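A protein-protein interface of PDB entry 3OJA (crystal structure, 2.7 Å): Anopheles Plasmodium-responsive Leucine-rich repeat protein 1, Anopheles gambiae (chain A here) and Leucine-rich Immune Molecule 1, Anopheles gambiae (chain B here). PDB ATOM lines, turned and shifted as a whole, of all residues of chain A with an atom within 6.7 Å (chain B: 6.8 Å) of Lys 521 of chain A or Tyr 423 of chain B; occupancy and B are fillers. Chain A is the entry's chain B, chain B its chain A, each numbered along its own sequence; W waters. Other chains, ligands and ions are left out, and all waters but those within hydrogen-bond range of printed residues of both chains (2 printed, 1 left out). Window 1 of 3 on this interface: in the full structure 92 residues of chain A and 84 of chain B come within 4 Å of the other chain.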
ATOM      1  N   LEU A 514     -17.998   6.699  -3.985  1.00  0.00           N
ATOM      2  CA  LEU A 514     -18.786   7.915  -4.022  1.00  0.00           C
ATOM      3  C   LEU A 514     -18.419   8.816  -5.189  1.00  0.00           C
ATOM      4  O   LEU A 514     -19.341   9.349  -5.816  1.00  0.00           O
ATOM      5  CB  LEU A 514     -18.681   8.671  -2.731  1.00  0.00           C
ATOM      6  CG  LEU A 514     -19.255   7.752  -1.682  1.00  0.00           C
ATOM      7  CD1 LEU A 514     -18.990   8.315  -0.314  1.00  0.00           C
ATOM      8  CD2 LEU A 514     -20.797   7.463  -1.899  1.00  0.00           C
ATOM      9  N   GLU A 516     -16.877   8.083  -8.128  1.00  0.00           N
ATOM     10  CA  GLU A 516     -17.319   7.475  -9.354  1.00  0.00           C
ATOM     11  C   GLU A 516     -18.797   7.702  -9.506  1.00  0.00           C
ATOM     12  O   GLU A 516     -19.235   8.061 -10.591  1.00  0.00           O
ATOM     13  CB  GLU A 516     -16.987   5.975  -9.417  1.00  0.00           C
ATOM     14  CG  GLU A 516     -15.493   5.770  -9.402  1.00  0.00           C
ATOM     15  CD  GLU A 516     -14.985   4.382  -9.819  1.00  0.00           C
ATOM     16  OE1 GLU A 516     -15.665   3.320  -9.591  1.00  0.00           O
ATOM     17  OE2 GLU A 516     -13.839   4.390 -10.360  1.00  0.00           O
ATOM     18  N   ARG A 517     -19.562   7.512  -8.431  1.00  0.00           N
ATOM     19  CA  ARG A 517     -20.992   7.639  -8.509  1.00  0.00           C
ATOM     20  C   ARG A 517     -21.372   9.046  -8.832  1.00  0.00           C
ATOM     21  O   ARG A 517     -22.129   9.223  -9.726  1.00  0.00           O
ATOM     22  CB  ARG A 517     -21.687   7.182  -7.241  1.00  0.00           C
ATOM     23  CG  ARG A 517     -23.190   7.008  -7.390  1.00  0.00           C
ATOM     24  CD  ARG A 517     -23.769   6.673  -6.091  1.00  0.00           C
ATOM     25  NE  ARG A 517     -23.595   7.717  -5.096  1.00  0.00           N
ATOM     26  CZ  ARG A 517     -24.336   7.806  -4.002  1.00  0.00           C
ATOM     27  NH1 ARG A 517     -25.284   6.915  -3.819  1.00  0.00           N
ATOM     28  NH2 ARG A 517     -24.153   8.757  -3.104  1.00  0.00           N
ATOM     29  N   GLN A 518     -20.859  10.042  -8.130  1.00  0.00           N
ATOM     30  CA  GLN A 518     -21.001  11.433  -8.562  1.00  0.00           C
ATOM     31  C   GLN A 518     -20.673  11.651 -10.062  1.00  0.00           C
ATOM     32  O   GLN A 518     -21.368  12.334 -10.761  1.00  0.00           O
ATOM     33  CB  GLN A 518     -20.088  12.345  -7.733  1.00  0.00           C
ATOM     34  CG  GLN A 518     -20.302  13.824  -7.922  1.00  0.00           C
ATOM     35  CD  GLN A 518     -21.750  14.232  -7.660  1.00  0.00           C
ATOM     36  OE1 GLN A 518     -22.427  13.672  -6.799  1.00  0.00           O
ATOM     37  NE2 GLN A 518     -22.241  15.208  -8.413  1.00  0.00           N
ATOM     38  N   ALA A 519     -19.610  11.081 -10.566  1.00  0.00           N
ATOM     39  CA  ALA A 519     -19.190  11.419 -11.920  1.00  0.00           C
ATOM     40  C   ALA A 519     -20.132  10.873 -12.991  1.00  0.00           C
ATOM     41  O   ALA A 519     -20.374  11.467 -14.058  1.00  0.00           O
ATOM     42  CB  ALA A 519     -17.777  10.900 -12.159  1.00  0.00           C
ATOM     43  N   PHE A 520     -20.632   9.701 -12.691  1.00  0.00           N
ATOM     44  CA  PHE A 520     -21.446   9.008 -13.606  1.00  0.00           C
ATOM     45  C   PHE A 520     -22.816   9.665 -13.558  1.00  0.00           C
ATOM     46  O   PHE A 520     -23.460   9.831 -14.602  1.00  0.00           O
ATOM     47  CB  PHE A 520     -21.541   7.556 -13.185  1.00  0.00           C
ATOM     48  CG  PHE A 520     -22.493   6.774 -13.981  1.00  0.00           C
ATOM     49  CD1 PHE A 520     -22.051   6.032 -15.051  1.00  0.00           C
ATOM     50  CD2 PHE A 520     -23.841   6.829 -13.696  1.00  0.00           C
ATOM     51  CE1 PHE A 520     -22.947   5.352 -15.795  1.00  0.00           C
ATOM     52  CE2 PHE A 520     -24.740   6.150 -14.444  1.00  0.00           C
ATOM     53  CZ  PHE A 520     -24.302   5.405 -15.480  1.00  0.00           C
ATOM     54  N   LYS A 521     -23.272  10.074 -12.378  1.00  0.00           N
ATOM     55  CA  LYS A 521     -24.497  10.795 -12.355  1.00  0.00           C
ATOM     56  C   LYS A 521     -24.388  12.119 -13.062  1.00  0.00           C
ATOM     57  O   LYS A 521     -25.329  12.550 -13.687  1.00  0.00           O
ATOM     58  CB  LYS A 521     -24.970  11.092 -10.963  1.00  0.00           C
ATOM     59  CG  LYS A 521     -26.436  11.463 -10.955  1.00  0.00           C
ATOM     60  CD  LYS A 521     -27.156  10.145 -10.831  1.00  0.00           C
ATOM     61  CE  LYS A 521     -28.368  10.184 -11.568  1.00  0.00           C
ATOM     62  NZ  LYS A 521     -28.984   8.919 -11.359  1.00  0.00           N
ATOM     63  N   LEU A 522     -23.282  12.800 -12.920  1.00  0.00           N
ATOM     64  CA  LEU A 522     -23.145  14.088 -13.562  1.00  0.00           C
ATOM     65  C   LEU A 522     -23.134  13.917 -15.099  1.00  0.00           C
ATOM     66  O   LEU A 522     -23.732  14.675 -15.826  1.00  0.00           O
ATOM     67  CB  LEU A 522     -21.854  14.765 -13.087  1.00  0.00           C
ATOM     68  CG  LEU A 522     -21.394  16.010 -13.821  1.00  0.00           C
ATOM     69  CD1 LEU A 522     -22.116  17.212 -13.203  1.00  0.00           C
ATOM     70  CD2 LEU A 522     -19.874  16.155 -13.745  1.00  0.00           C
ATOM     71  N   ARG A 523     -22.455  12.904 -15.595  1.00  0.00           N
ATOM     72  CA  ARG A 523     -22.322  12.768 -17.025  1.00  0.00           C
ATOM     73  C   ARG A 523     -23.701  12.463 -17.592  1.00  0.00           C
ATOM     74  O   ARG A 523     -24.100  13.029 -18.610  1.00  0.00           O
ATOM     75  CB  ARG A 523     -21.363  11.628 -17.321  1.00  0.00           C
ATOM     76  CG  ARG A 523     -20.956  11.512 -18.738  1.00  0.00           C
ATOM     77  CD  ARG A 523     -19.999  10.344 -18.943  1.00  0.00           C
ATOM     78  NE  ARG A 523     -19.665  10.245 -20.369  1.00  0.00           N
ATOM     79  CZ  ARG A 523     -18.843  11.078 -21.030  1.00  0.00           C
ATOM     80  NH1 ARG A 523     -18.219  12.098 -20.411  1.00  0.00           N
ATOM     81  NH2 ARG A 523     -18.639  10.880 -22.331  1.00  0.00           N
ATOM     82  N   GLU A 524     -24.422  11.572 -16.910  1.00  0.00           N
ATOM     83  CA  GLU A 524     -25.794  11.274 -17.235  1.00  0.00           C
ATOM     84  C   GLU A 524     -26.710  12.513 -17.308  1.00  0.00           C
ATOM     85  O   GLU A 524     -27.556  12.611 -18.219  1.00  0.00           O
ATOM     86  CB  GLU A 524     -26.332  10.299 -16.221  1.00  0.00           C
ATOM     87  CG  GLU A 524     -27.437   9.385 -16.694  1.00  0.00           C
ATOM     88  CD  GLU A 524     -27.976   8.503 -15.524  1.00  0.00           C
ATOM     89  OE1 GLU A 524     -28.324   9.074 -14.453  1.00  0.00           O
ATOM     90  OE2 GLU A 524     -28.027   7.240 -15.669  1.00  0.00           O
ATOM     91  N   THR A 525     -26.576  13.439 -16.364  1.00  0.00           N
ATOM     92  CA  THR A 525     -27.400  14.643 -16.380  1.00  0.00           C
ATOM     93  C   THR A 525     -27.027  15.562 -17.539  1.00  0.00           C
ATOM     94  O   THR A 525     -27.877  16.129 -18.215  1.00  0.00           O
ATOM     95  CB  THR A 525     -27.214  15.391 -15.122  1.00  0.00           C
ATOM     96  OG1 THR A 525     -27.440  14.492 -14.068  1.00  0.00           O
ATOM     97  CG2 THR A 525     -28.183  16.540 -15.001  1.00  0.00           C
ATOM     98  N   GLN A 526     -25.733  15.710 -17.753  1.00  0.00           N
ATOM     99  CA  GLN A 526     -25.242  16.470 -18.856  1.00  0.00           C
ATOM    100  C   GLN A 526     -25.897  15.923 -20.121  1.00  0.00           C
ATOM    101  O   GLN A 526     -26.330  16.675 -20.991  1.00  0.00           O
ATOM    102  CB  GLN A 526     -23.729  16.347 -18.909  1.00  0.00           C
ATOM    103  CG  GLN A 526     -23.005  17.365 -18.075  1.00  0.00           C
ATOM    104  CD  GLN A 526     -21.564  16.963 -17.773  1.00  0.00           C
ATOM    105  OE1 GLN A 526     -21.212  15.774 -17.908  1.00  0.00           O
ATOM    106  NE2 GLN A 526     -20.720  17.941 -17.390  1.00  0.00           N
ATOM    107  N   ARG B 418     -21.867  14.791   2.667  1.00  0.00           N
ATOM    108  CA  ARG B 418     -21.763  15.772   1.594  1.00  0.00           C
ATOM    109  C   ARG B 418     -21.933  15.121   0.219  1.00  0.00           C
ATOM    110  O   ARG B 418     -22.642  15.630  -0.626  1.00  0.00           O
ATOM    111  CB  ARG B 418     -20.439  16.503   1.697  1.00  0.00           C
ATOM    112  CG  ARG B 418     -20.171  17.524   0.643  1.00  0.00           C
ATOM    113  CD  ARG B 418     -21.210  18.594   0.632  1.00  0.00           C
ATOM    114  NE  ARG B 418     -20.981  19.494  -0.503  1.00  0.00           N
ATOM    115  CZ  ARG B 418     -21.944  20.181  -1.106  1.00  0.00           C
ATOM    116  NH1 ARG B 418     -23.196  20.076  -0.696  1.00  0.00           N
ATOM    117  NH2 ARG B 418     -21.679  20.946  -2.145  1.00  0.00           N
ATOM    118  N   TYR B 419     -21.333  13.967   0.012  1.00  0.00           N
ATOM    119  CA  TYR B 419     -21.515  13.283  -1.223  1.00  0.00           C
ATOM    120  C   TYR B 419     -23.003  12.978  -1.401  1.00  0.00           C
ATOM    121  O   TYR B 419     -23.494  13.048  -2.496  1.00  0.00           O
ATOM    122  CB  TYR B 419     -20.684  12.002  -1.250  1.00  0.00           C
ATOM    123  CG  TYR B 419     -19.290  12.218  -1.748  1.00  0.00           C
ATOM    124  CD1 TYR B 419     -19.029  12.374  -3.078  1.00  0.00           C
ATOM    125  CD2 TYR B 419     -18.219  12.259  -0.890  1.00  0.00           C
ATOM    126  CE1 TYR B 419     -17.753  12.548  -3.543  1.00  0.00           C
ATOM    127  CE2 TYR B 419     -16.939  12.424  -1.353  1.00  0.00           C
ATOM    128  CZ  TYR B 419     -16.712  12.568  -2.680  1.00  0.00           C
ATOM    129  OH  TYR B 419     -15.430  12.763  -3.141  1.00  0.00           O
ATOM    130  N   GLU B 420     -23.713  12.618  -0.334  1.00  0.00           N
ATOM    131  CA  GLU B 420     -25.129  12.319  -0.433  1.00  0.00           C
ATOM    132  C   GLU B 420     -25.901  13.567  -0.830  1.00  0.00           C
ATOM    133  O   GLU B 420     -26.723  13.498  -1.725  1.00  0.00           O
ATOM    134  CB  GLU B 420     -25.690  11.779   0.871  1.00  0.00           C
ATOM    135  CG  GLU B 420     -25.281  10.370   1.183  1.00  0.00           C
ATOM    136  CD  GLU B 420     -25.733   9.384   0.142  1.00  0.00           C
ATOM    137  OE1 GLU B 420     -26.915   9.528  -0.286  1.00  0.00           O
ATOM    138  OE2 GLU B 420     -24.937   8.457  -0.205  1.00  0.00           O
ATOM    139  N   GLU B 421     -25.649  14.709  -0.193  1.00  0.00           N
ATOM    140  CA  GLU B 421     -26.222  15.980  -0.674  1.00  0.00           C
ATOM    141  C   GLU B 421     -25.964  16.242  -2.198  1.00  0.00           C
ATOM    142  O   GLU B 421     -26.773  16.823  -2.906  1.00  0.00           O
ATOM    143  CB  GLU B 421     -25.633  17.156   0.103  1.00  0.00           C
ATOM    144  CG  GLU B 421     -26.260  17.473   1.421  1.00  0.00           C
ATOM    145  CD  GLU B 421     -25.463  18.537   2.199  1.00  0.00           C
ATOM    146  OE1 GLU B 421     -24.255  18.746   1.941  1.00  0.00           O
ATOM    147  OE2 GLU B 421     -26.040  19.171   3.092  1.00  0.00           O
ATOM    148  N   MET B 422     -24.797  15.865  -2.677  1.00  0.00           N
ATOM    149  CA  MET B 422     -24.360  16.295  -3.954  1.00  0.00           C
ATOM    150  C   MET B 422     -25.093  15.473  -4.955  1.00  0.00           C
ATOM    151  O   MET B 422     -25.593  16.027  -5.947  1.00  0.00           O
ATOM    152  CB  MET B 422     -22.852  16.107  -4.089  1.00  0.00           C
ATOM    153  CG  MET B 422     -22.080  17.235  -3.462  1.00  0.00           C
ATOM    154  SD  MET B 422     -20.355  16.922  -3.223  1.00  0.00           S
ATOM    155  CE  MET B 422     -19.854  15.968  -4.656  1.00  0.00           C
ATOM    156  N   TYR B 423     -25.149  14.156  -4.674  1.00  0.00           N
ATOM    157  CA  TYR B 423     -25.893  13.193  -5.447  1.00  0.00           C
ATOM    158  C   TYR B 423     -27.370  13.594  -5.591  1.00  0.00           C
ATOM    159  O   TYR B 423     -27.913  13.612  -6.679  1.00  0.00           O
ATOM    160  CB  TYR B 423     -25.865  11.874  -4.748  1.00  0.00           C
ATOM    161  CG  TYR B 423     -26.322  10.747  -5.608  1.00  0.00           C
ATOM    162  CD1 TYR B 423     -25.604  10.391  -6.708  1.00  0.00           C
ATOM    163  CD2 TYR B 423     -27.466  10.050  -5.328  1.00  0.00           C
ATOM    164  CE1 TYR B 423     -25.985   9.369  -7.517  1.00  0.00           C
ATOM    165  CE2 TYR B 423     -27.873   9.004  -6.120  1.00  0.00           C
ATOM    166  CZ  TYR B 423     -27.123   8.658  -7.216  1.00  0.00           C
ATOM    167  OH  TYR B 423     -27.470   7.614  -8.044  1.00  0.00           O
ATOM    168  N   VAL B 424     -28.026  13.870  -4.478  1.00  0.00           N
ATOM    169  CA  VAL B 424     -29.340  14.381  -4.524  1.00  0.00           C
ATOM    170  C   VAL B 424     -29.407  15.673  -5.367  1.00  0.00           C
ATOM    171  O   VAL B 424     -30.285  15.752  -6.231  1.00  0.00           O
ATOM    172  CB  VAL B 424     -29.904  14.519  -3.118  1.00  0.00           C
ATOM    173  CG1 VAL B 424     -30.954  15.598  -3.040  1.00  0.00           C
ATOM    174  CG2 VAL B 424     -30.492  13.216  -2.674  1.00  0.00           C
ATOM    175  N   GLU B 425     -28.518  16.655  -5.179  1.00  0.00           N
ATOM    176  CA  GLU B 425     -28.547  17.875  -6.022  1.00  0.00           C
ATOM    177  C   GLU B 425     -28.494  17.445  -7.470  1.00  0.00           C
ATOM    178  O   GLU B 425     -29.246  17.927  -8.292  1.00  0.00           O
ATOM    179  CB  GLU B 425     -27.386  18.873  -5.749  1.00  0.00           C
ATOM    180  CG  GLU B 425     -27.678  19.973  -4.662  1.00  0.00           C
ATOM    181  CD  GLU B 425     -26.398  20.424  -3.835  1.00  0.00           C
ATOM    182  OE1 GLU B 425     -25.266  20.317  -4.408  1.00  0.00           O
ATOM    183  OE2 GLU B 425     -26.514  20.867  -2.627  1.00  0.00           O
ATOM    184  N   GLN B 426     -27.619  16.506  -7.792  1.00  0.00           N
ATOM    185  CA  GLN B 426     -27.354  16.212  -9.188  1.00  0.00           C
ATOM    186  C   GLN B 426     -28.618  15.619  -9.749  1.00  0.00           C
ATOM    187  O   GLN B 426     -28.994  15.945 -10.864  1.00  0.00           O
ATOM    188  CB  GLN B 426     -26.160  15.263  -9.362  1.00  0.00           C
ATOM    189  CG  GLN B 426     -25.462  15.341 -10.674  1.00  0.00           C
ATOM    190  CD  GLN B 426     -25.198  16.778 -11.134  1.00  0.00           C
ATOM    191  OE1 GLN B 426     -25.647  17.196 -12.222  1.00  0.00           O
ATOM    192  NE2 GLN B 426     -24.467  17.533 -10.317  1.00  0.00           N
ATOM    193  N   GLN B 427     -29.298  14.796  -8.964  1.00  0.00           N
ATOM    194  CA  GLN B 427     -30.484  14.065  -9.386  1.00  0.00           C
ATOM    195  C   GLN B 427     -31.635  15.035  -9.604  1.00  0.00           C
ATOM    196  O   GLN B 427     -32.440  14.926 -10.510  1.00  0.00           O
ATOM    197  CB  GLN B 427     -30.807  13.043  -8.298  1.00  0.00           C
ATOM    198  CG  GLN B 427     -31.810  12.004  -8.628  1.00  0.00           C
ATOM    199  CD  GLN B 427     -31.579  11.277  -9.962  1.00  0.00           C
ATOM    200  OE1 GLN B 427     -30.713  10.381 -10.054  1.00  0.00           O
ATOM    201  NE2 GLN B 427     -32.424  11.605 -10.994  1.00  0.00           N
ATOM    202  N   SER B 428     -31.690  16.051  -8.794  1.00  0.00           N
ATOM    203  CA  SER B 428     -32.740  17.014  -8.947  1.00  0.00           C
ATOM    204  C   SER B 428     -32.539  17.837 -10.265  1.00  0.00           C
ATOM    205  O   SER B 428     -33.497  18.154 -11.028  1.00  0.00           O
ATOM    206  CB  SER B 428     -32.719  17.851  -7.727  1.00  0.00           C
ATOM    207  OG  SER B 428     -33.425  19.016  -7.964  1.00  0.00           O
ATOM    208  N   GLN B 430     -31.020  16.709 -12.909  1.00  0.00           N
ATOM    209  CA  GLN B 430     -31.375  15.793 -13.985  1.00  0.00           C
ATOM    210  C   GLN B 430     -32.873  15.708 -14.183  1.00  0.00           C
ATOM    211  O   GLN B 430     -33.353  15.758 -15.278  1.00  0.00           O
ATOM    212  CB  GLN B 430     -30.812  14.422 -13.725  1.00  0.00           C
ATOM    213  CG  GLN B 430     -31.194  13.463 -14.751  1.00  0.00           C
ATOM    214  CD  GLN B 430     -30.550  12.077 -14.591  1.00  0.00           C
ATOM    215  OE1 GLN B 430     -31.159  11.045 -14.928  1.00  0.00           O
ATOM    216  NE2 GLN B 430     -29.293  12.050 -14.137  1.00  0.00           N
HETATM  217  O   HOH W   1     -23.835  17.880  -7.581  1.00  0.00           O
HETATM  218  O   HOH W   2     -27.132   7.287  -1.354  1.00  0.00           O
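N of Tyr 423 of chain B sits at hydrogen-bond distance from OE1 of Gln 518 of chain A (3.5 Å). The side-chain carboxylate of Glu 420 of chain B is in salt-bridge range of the guanidinium group of Arg 517 of chain A, 3.0 Å away. The side-chain amide nitrogen (NE2) of Gln 430 of chain B sits at hydrogen-bond distance from the side-chain hydroxyl (OG1) of Thr 525 of chain A (3.1 Å). The side-chain amino group (NZ) of Lys 521 of chain A is in hydrogen-bond range of the side-chain amide oxygen (OE1) of Gln 427 of chain B (2.6 Å). The side-chain carboxylate (OE1) of Glu 524 of chain A sits at hydrogen-bond distance from the side-chain amide nitrogen (NE2) of Gln 430 of chain B (3.1 Å).
The side-chain amino group of Lys 521 of chain A is in salt-bridge range of the side-chain carboxylate of Glu 524 of chain A (3.2 Å). The backbone carbonyl oxygen (O) of Leu 522 of chain A lies close to the side-chain amide oxygen (OE1) of Gln 526 of chain A (3.4 Å). The guanidinium group (NE) of Arg 418 of chain B lies within hydrogen-bond range of the side-chain sulfur (SD) of Met 422 of chain B, 3.8 Å away. The side-chain hydroxyl (OG1) of Thr 525 of chain A sits at hydrogen-bond distance from the backbone carbonyl oxygen (O) of Lys 521 of chain A (2.9 Å).
Among the printed residues, pairs that only touch across the chains: Leu 514 of chain A with Tyr 419 of chain B, Arg 517 of chain A with Tyr 423 of chain B, Gln 518 of chain A with Met 422 of chain B, Gln 518 of chain A with Gln 426 of chain B, Lys 521 of chain A with Tyr 423 of chain B, Lys 521 of chain A with Gln 430 of chain B, Leu 522 of chain A with Gln 426 of chain B and Thr 525 of chain A with Gln 426 of chain B.
Printed residues of chain B within 4 Å of Gln 518 of chain A: Met 422, Tyr 423 and Gln 426. Printed residues of chain B within 4 Å of Lys 521 of chain A: Tyr 423 (3.6 Å), Gln 427 (2.6 Å) and Gln 430 (3.3 Å). Printed residues of chain B within 4 Å of Leu 522 of chain A: Gln 426 (3.7 Å). Tyr 423 of chain B touches just these residues of chain A: Arg 517, Gln 518 and Lys 521. The nearest printed residue of chain B that does not touch Lys 521 of chain A is Gln 426 of chain B (4.01 Å).
Of the 12 printed residues of chain B, 7 touch a printed residue of chain A. Among the printed residues, Asp or Glu carboxylates within 4 Å of a Lys or Arg side-chain nitrogen of the other chain: Arg 517 of chain A with Glu 420 of chain B (3.0 Å).
Water W2 lies within hydrogen-bond range of OE1 of Glu 420 of chain B (2.5 Å) and NH1 of Arg 517 of chain A (3.1 Å). Water W1 lies within hydrogen-bond range of the side-chain amide nitrogen (NE2) of Gln 426 of chain B, the backbone carbonyl oxygen (O) of Met 422 of chain B and the side-chain amide nitrogen (NE2) of Gln 518 of chain A.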
